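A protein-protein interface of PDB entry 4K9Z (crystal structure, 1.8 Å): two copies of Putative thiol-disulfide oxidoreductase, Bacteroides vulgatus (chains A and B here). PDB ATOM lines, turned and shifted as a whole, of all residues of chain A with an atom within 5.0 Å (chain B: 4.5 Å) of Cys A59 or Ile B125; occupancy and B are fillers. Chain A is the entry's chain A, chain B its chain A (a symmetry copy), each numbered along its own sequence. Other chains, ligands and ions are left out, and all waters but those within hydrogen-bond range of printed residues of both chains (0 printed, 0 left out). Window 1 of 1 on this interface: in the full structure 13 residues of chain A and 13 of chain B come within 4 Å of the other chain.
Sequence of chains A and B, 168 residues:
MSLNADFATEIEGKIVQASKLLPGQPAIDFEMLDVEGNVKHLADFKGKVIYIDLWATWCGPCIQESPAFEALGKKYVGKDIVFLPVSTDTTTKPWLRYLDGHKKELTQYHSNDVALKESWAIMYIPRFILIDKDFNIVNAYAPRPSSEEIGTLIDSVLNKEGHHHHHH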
ATOM      1  N   ALA A  56     -18.480 -22.316  -4.455  1.00  0.00           N
ATOM      2  CA  ALA A  56     -17.969 -21.366  -5.448  1.00  0.00           C
ATOM      3  C   ALA A  56     -16.949 -20.465  -4.776  1.00  0.00           C
ATOM      4  O   ALA A  56     -16.970 -20.301  -3.565  1.00  0.00           O
ATOM      5  CB  ALA A  56     -19.088 -20.549  -6.059  1.00  0.00           C
ATOM      6  N   THR A  57     -16.050 -19.884  -5.572  1.00  0.00           N
ATOM      7  CA  THR A  57     -14.918 -19.147  -5.021  1.00  0.00           C
ATOM      8  C   THR A  57     -15.324 -17.901  -4.253  1.00  0.00           C
ATOM      9  O   THR A  57     -14.560 -17.410  -3.423  1.00  0.00           O
ATOM     10  CB  THR A  57     -13.936 -18.723  -6.140  1.00  0.00           C
ATOM     11  OG1 THR A  57     -14.635 -17.905  -7.080  1.00  0.00           O
ATOM     12  CG2 THR A  57     -13.402 -19.954  -6.862  1.00  0.00           C
ATOM     13  N   TRP A  58     -16.506 -17.363  -4.539  1.00  0.00           N
ATOM     14  CA  TRP A  58     -16.968 -16.178  -3.814  1.00  0.00           C
ATOM     15  C   TRP A  58     -17.964 -16.498  -2.693  1.00  0.00           C
ATOM     16  O   TRP A  58     -18.494 -15.598  -2.042  1.00  0.00           O
ATOM     17  CB  TRP A  58     -17.507 -15.089  -4.767  1.00  0.00           C
ATOM     18  CG  TRP A  58     -18.418 -15.553  -5.880  1.00  0.00           C
ATOM     19  CD1 TRP A  58     -18.458 -16.793  -6.458  1.00  0.00           C
ATOM     20  CD2 TRP A  58     -19.412 -14.770  -6.555  1.00  0.00           C
ATOM     21  NE1 TRP A  58     -19.416 -16.831  -7.434  1.00  0.00           N
ATOM     22  CE2 TRP A  58     -20.017 -15.603  -7.517  1.00  0.00           C
ATOM     23  CE3 TRP A  58     -19.852 -13.449  -6.435  1.00  0.00           C
ATOM     24  CZ2 TRP A  58     -21.040 -15.157  -8.353  1.00  0.00           C
ATOM     25  CZ3 TRP A  58     -20.867 -13.010  -7.263  1.00  0.00           C
ATOM     26  CH2 TRP A  58     -21.449 -13.860  -8.211  1.00  0.00           C
ATOM     27  N   CYS A  59     -18.199 -17.788  -2.459  1.00  0.00           N
ATOM     28  CA  CYS A  59     -19.099 -18.211  -1.373  1.00  0.00           C
ATOM     29  C   CYS A  59     -18.331 -18.409  -0.065  1.00  0.00           C
ATOM     30  O   CYS A  59     -17.719 -19.451   0.153  1.00  0.00           O
ATOM     31  CB  CYS A  59     -19.800 -19.524  -1.779  1.00  0.00           C
ATOM     32  SG  CYS A  59     -20.916 -20.205  -0.517  1.00  0.00           S
ATOM     33  N   GLY A  60     -18.349 -17.408   0.810  1.00  0.00           N
ATOM     34  CA  GLY A  60     -17.609 -17.495   2.063  1.00  0.00           C
ATOM     35  C   GLY A  60     -17.973 -18.714   2.891  1.00  0.00           C
ATOM     36  O   GLY A  60     -17.096 -19.469   3.314  1.00  0.00           O
ATOM     37  N   PRO A  61     -19.272 -18.920   3.115  1.00  0.00           N
ATOM     38  CA  PRO A  61     -19.665 -20.053   3.956  1.00  0.00           C
ATOM     39  C   PRO A  61     -19.316 -21.408   3.322  1.00  0.00           C
ATOM     40  O   PRO A  61     -19.087 -22.374   4.069  1.00  0.00           O
ATOM     41  CB  PRO A  61     -21.182 -19.872   4.070  1.00  0.00           C
ATOM     42  CG  PRO A  61     -21.366 -18.363   3.982  1.00  0.00           C
ATOM     43  CD  PRO A  61     -20.398 -17.988   2.893  1.00  0.00           C
ATOM     44  N   CYS A  62     -19.262 -21.482   1.992  1.00  0.00           N
ATOM     45  CA  CYS A  62     -18.839 -22.713   1.320  1.00  0.00           C
ATOM     46  C   CYS A  62     -17.390 -23.005   1.667  1.00  0.00           C
ATOM     47  O   CYS A  62     -17.037 -24.128   2.017  1.00  0.00           O
ATOM     48  CB  CYS A  62     -18.957 -22.584  -0.213  1.00  0.00           C
ATOM     49  SG  CYS A  62     -20.627 -22.241  -0.844  1.00  0.00           S
ATOM     50  N   ILE A  63     -16.544 -21.983   1.559  1.00  0.00           N
ATOM     51  CA  ILE A  63     -15.124 -22.158   1.829  1.00  0.00           C
ATOM     52  C   ILE A  63     -14.875 -22.464   3.310  1.00  0.00           C
ATOM     53  O   ILE A  63     -13.918 -23.152   3.659  1.00  0.00           O
ATOM     54  CB  ILE A  63     -14.310 -20.954   1.287  1.00  0.00           C
ATOM     55  CG1 ILE A  63     -14.319 -21.013  -0.249  1.00  0.00           C
ATOM     56  CG2 ILE A  63     -12.867 -20.969   1.801  1.00  0.00           C
ATOM     57  CD1 ILE A  63     -14.113 -19.701  -0.931  1.00  0.00           C
ATOM     58  N   ILE A 125     -26.162 -22.498  -2.665  1.00  0.00           N
ATOM     59  CA  ILE A 125     -25.012 -23.165  -2.054  1.00  0.00           C
ATOM     60  C   ILE A 125     -24.722 -22.423  -0.755  1.00  0.00           C
ATOM     61  O   ILE A 125     -25.146 -21.281  -0.597  1.00  0.00           O
ATOM     62  CB  ILE A 125     -23.761 -23.155  -2.963  1.00  0.00           C
ATOM     63  CG1 ILE A 125     -23.420 -21.736  -3.405  1.00  0.00           C
ATOM     64  CG2 ILE A 125     -23.961 -24.049  -4.179  1.00  0.00           C
ATOM     65  CD1 ILE A 125     -22.178 -21.692  -4.341  1.00  0.00           C
ATOM     66  N   PRO A 126     -24.009 -23.061   0.190  1.00  0.00           N
ATOM     67  CA  PRO A 126     -23.470 -24.429   0.212  1.00  0.00           C
ATOM     68  C   PRO A 126     -24.567 -25.466   0.048  1.00  0.00           C
ATOM     69  O   PRO A 126     -25.705 -25.307   0.543  1.00  0.00           O
ATOM     70  CB  PRO A 126     -22.894 -24.564   1.632  1.00  0.00           C
ATOM     71  CG  PRO A 126     -22.630 -23.152   2.057  1.00  0.00           C
ATOM     72  CD  PRO A 126     -23.745 -22.346   1.451  1.00  0.00           C
ATOM     73  N   LEU B  54     -24.335  -7.058   0.357  1.00  0.00           N
ATOM     74  CA  LEU B  54     -23.894  -7.668  -0.891  1.00  0.00           C
ATOM     75  C   LEU B  54     -24.288  -9.127  -0.878  1.00  0.00           C
ATOM     76  O   LEU B  54     -23.835  -9.882  -0.022  1.00  0.00           O
ATOM     77  CB  LEU B  54     -22.382  -7.538  -1.004  1.00  0.00           C
ATOM     78  CG  LEU B  54     -22.005  -6.073  -1.224  1.00  0.00           C
ATOM     79  CD1 LEU B  54     -20.595  -5.842  -0.731  1.00  0.00           C
ATOM     80  CD2 LEU B  54     -22.144  -5.665  -2.695  1.00  0.00           C
ATOM     81  N   TRP B  55     -25.140  -9.527  -1.822  1.00  0.00           N
ATOM     82  CA  TRP B  55     -25.696 -10.876  -1.787  1.00  0.00           C
ATOM     83  C   TRP B  55     -25.740 -11.383  -3.227  1.00  0.00           C
ATOM     84  O   TRP B  55     -25.384 -10.653  -4.155  1.00  0.00           O
ATOM     85  CB  TRP B  55     -27.110 -10.833  -1.191  1.00  0.00           C
ATOM     86  CG  TRP B  55     -28.133 -10.133  -2.087  1.00  0.00           C
ATOM     87  CD1 TRP B  55     -28.255  -8.792  -2.306  1.00  0.00           C
ATOM     88  CD2 TRP B  55     -29.179 -10.758  -2.839  1.00  0.00           C
ATOM     89  NE1 TRP B  55     -29.315  -8.536  -3.164  1.00  0.00           N
ATOM     90  CE2 TRP B  55     -29.894  -9.736  -3.502  1.00  0.00           C
ATOM     91  CE3 TRP B  55     -29.583 -12.091  -3.008  1.00  0.00           C
ATOM     92  CZ2 TRP B  55     -30.990 -10.004  -4.336  1.00  0.00           C
ATOM     93  CZ3 TRP B  55     -30.673 -12.359  -3.838  1.00  0.00           C
ATOM     94  CH2 TRP B  55     -31.365 -11.313  -4.488  1.00  0.00           C
ATOM     95  N   ALA B  56     -26.151 -12.636  -3.407  1.00  0.00           N
ATOM     96  CA  ALA B  56     -26.447 -13.163  -4.742  1.00  0.00           C
ATOM     97  C   ALA B  56     -27.541 -14.209  -4.620  1.00  0.00           C
ATOM     98  O   ALA B  56     -27.730 -14.785  -3.558  1.00  0.00           O
ATOM     99  CB  ALA B  56     -25.212 -13.751  -5.391  1.00  0.00           C
ATOM    100  N   CYS B  59     -26.636 -17.565  -3.199  1.00  0.00           N
ATOM    101  CA  CYS B  59     -25.958 -17.575  -1.892  1.00  0.00           C
ATOM    102  C   CYS B  59     -26.951 -17.822  -0.756  1.00  0.00           C
ATOM    103  O   CYS B  59     -27.626 -16.901  -0.300  1.00  0.00           O
ATOM    104  CB  CYS B  59     -25.238 -16.227  -1.683  1.00  0.00           C
ATOM    105  SG  CYS B  59     -24.387 -16.065  -0.086  1.00  0.00           S
ATOM    106  N   CYS B  62     -26.500 -15.690   2.374  1.00  0.00           N
ATOM    107  CA  CYS B  62     -26.836 -14.289   2.110  1.00  0.00           C
ATOM    108  C   CYS B  62     -28.333 -14.091   2.274  1.00  0.00           C
ATOM    109  O   CYS B  62     -28.779 -13.149   2.924  1.00  0.00           O
ATOM    110  CB  CYS B  62     -26.444 -13.879   0.676  1.00  0.00           C
ATOM    111  SG  CYS B  62     -24.678 -14.035   0.272  1.00  0.00           S
ATOM    112  N   THR B  88     -24.791  -9.216  -6.537  1.00  0.00           N
ATOM    113  CA  THR B  88     -23.555  -9.327  -7.297  1.00  0.00           C
ATOM    114  C   THR B  88     -23.644 -10.471  -8.311  1.00  0.00           C
ATOM    115  O   THR B  88     -22.617 -10.970  -8.772  1.00  0.00           O
ATOM    116  CB  THR B  88     -22.335  -9.549  -6.375  1.00  0.00           C
ATOM    117  OG1 THR B  88     -22.500 -10.770  -5.641  1.00  0.00           O
ATOM    118  CG2 THR B  88     -22.193  -8.395  -5.400  1.00  0.00           C
ATOM    119  N   ILE B 122     -14.139  -7.035  -2.443  1.00  0.00           N
ATOM    120  CA  ILE B 122     -15.231  -7.981  -2.243  1.00  0.00           C
ATOM    121  C   ILE B 122     -14.880  -9.307  -2.893  1.00  0.00           C
ATOM    122  O   ILE B 122     -15.097  -9.531  -4.088  1.00  0.00           O
ATOM    123  CB  ILE B 122     -16.569  -7.395  -2.708  1.00  0.00           C
ATOM    124  CG1 ILE B 122     -16.873  -6.170  -1.840  1.00  0.00           C
ATOM    125  CG2 ILE B 122     -17.698  -8.428  -2.559  1.00  0.00           C
ATOM    126  CD1 ILE B 122     -17.761  -5.151  -2.501  1.00  0.00           C
ATOM    127  N   TYR B 124     -15.532 -12.367  -1.007  1.00  0.00           N
ATOM    128  CA  TYR B 124     -16.522 -13.343  -0.563  1.00  0.00           C
ATOM    129  C   TYR B 124     -17.798 -12.649  -0.147  1.00  0.00           C
ATOM    130  O   TYR B 124     -17.765 -11.516   0.338  1.00  0.00           O
ATOM    131  CB  TYR B 124     -16.012 -14.153   0.629  1.00  0.00           C
ATOM    132  CG  TYR B 124     -14.650 -14.771   0.423  1.00  0.00           C
ATOM    133  CD1 TYR B 124     -14.493 -15.926  -0.333  1.00  0.00           C
ATOM    134  CD2 TYR B 124     -13.519 -14.197   0.990  1.00  0.00           C
ATOM    135  CE1 TYR B 124     -13.234 -16.487  -0.518  1.00  0.00           C
ATOM    136  CE2 TYR B 124     -12.263 -14.752   0.809  1.00  0.00           C
ATOM    137  CZ  TYR B 124     -12.126 -15.892   0.056  1.00  0.00           C
ATOM    138  OH  TYR B 124     -10.867 -16.434  -0.118  1.00  0.00           O
ATOM    139  N   ILE B 125     -18.919 -13.337  -0.331  1.00  0.00           N
ATOM    140  CA  ILE B 125     -20.180 -12.888   0.259  1.00  0.00           C
ATOM    141  C   ILE B 125     -20.672 -14.027   1.144  1.00  0.00           C
ATOM    142  O   ILE B 125     -20.247 -15.165   0.966  1.00  0.00           O
ATOM    143  CB  ILE B 125     -21.249 -12.540  -0.803  1.00  0.00           C
ATOM    144  CG1 ILE B 125     -21.461 -13.705  -1.766  1.00  0.00           C
ATOM    145  CG2 ILE B 125     -20.865 -11.286  -1.575  1.00  0.00           C
ATOM    146  CD1 ILE B 125     -22.514 -13.379  -2.863  1.00  0.00           C
ATOM    147  N   PRO B 126     -21.562 -13.736   2.109  1.00  0.00           N
ATOM    148  CA  PRO B 126     -22.140 -12.444   2.511  1.00  0.00           C
ATOM    149  C   PRO B 126     -21.066 -11.452   2.916  1.00  0.00           C
ATOM    150  O   PRO B 126     -20.029 -11.809   3.518  1.00  0.00           O
ATOM    151  CB  PRO B 126     -22.964 -12.795   3.762  1.00  0.00           C
ATOM    152  CG  PRO B 126     -23.253 -14.257   3.615  1.00  0.00           C
ATOM    153  CD  PRO B 126     -22.023 -14.837   2.974  1.00  0.00           C
ATOM    154  N   ARG B 127     -21.318 -10.200   2.566  1.00  0.00           N
ATOM    155  CA  ARG B 127     -20.434  -9.096   2.899  1.00  0.00           C
ATOM    156  C   ARG B 127     -21.316  -7.898   3.157  1.00  0.00           C
ATOM    157  O   ARG B 127     -22.259  -7.632   2.389  1.00  0.00           O
ATOM    158  CB  ARG B 127     -19.473  -8.817   1.740  1.00  0.00           C
ATOM    159  CG  ARG B 127     -18.633  -7.557   1.941  1.00  0.00           C
ATOM    160  CD  ARG B 127     -17.475  -7.732   2.953  1.00  0.00           C
ATOM    161  NE  ARG B 127     -16.712  -6.488   2.949  1.00  0.00           N
ATOM    162  CZ  ARG B 127     -15.712  -6.228   2.110  1.00  0.00           C
ATOM    163  NH1 ARG B 127     -15.297  -7.157   1.254  1.00  0.00           N
ATOM    164  NH2 ARG B 127     -15.109  -5.051   2.152  1.00  0.00           N
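The backbone carbonyl oxygen (O) of Trp A58 sits at hydrogen-bond distance from the backbone NH (N) of Ile B125 (2.9 Å). O of Ile B125 is in hydrogen-bond range of N of Gly A60 (2.9 Å).
Of the printed residues of chain B, Cys A59 touches Ile B125. Printed residues of chain A within 4 Å of Ile B125: Trp A58 (2.9 Å), Cys A59 (3.9 Å), Gly A60 (2.9 Å) and Pro A61 (3.4 Å). Printed residues of chain A within 4 Å of Thr B88: Trp A58 (3.1 Å). Printed residues of chain A within 4 Å of Pro B126: Pro A61. Of the printed residues of chain B, Ile A125 touches Cys B59 (3.9 Å). Ala B56 touches none of the printed residues of chain A. The nearest printed residue of chain A that does not touch Ile B125 is Cys A62 (6.5 Å). The nearest printed residue of chain B that does not touch Ile A125 is Cys B62 (6.5 Å).
Of the 11 printed residues of chain B, 5 touch a printed residue of chain A. Printed residues of chain B that touch a printed residue of chain A: Cys B59, Thr B88, Tyr B124, Ile B125 and Pro B126. Of the 10 printed residues of chain A, 7 touch a printed residue of chain B. Among the printed residues, 11 pairs touch across the chains. Among the printed residues, no Asp or Glu carboxylate lies within 4 Å of a Lys or Arg side-chain nitrogen of the other chain.
O of Trp B55 lies within hydrogen-bond range of N of Thr B88 (2.8 Å). The side-chain sulfur (SG) of Cys A59 is disulfide-bonded to the side-chain sulfur (SG) of Cys A62 (2.1 Å). The side-chain sulfur (SG) of Cys B59 is disulfide-bonded to the side-chain sulfur (SG) of Cys B62 (2.1 Å).
Cys A59 touches Ile B125, and with the chains exchanged Ile A125 touches Cys B59.
Among the printed residues, merely in contact across the chains: Trp A58 with Thr B88, Thr A57 with Tyr B124, Trp A58 with Tyr B124, Ile A63 with Tyr B124, Pro A61 with Ile B125, Pro A61 with Pro B126, Ile A125 with Cys B59, Cys A59 with Ile B125 and Gly A60 with Tyr B124.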
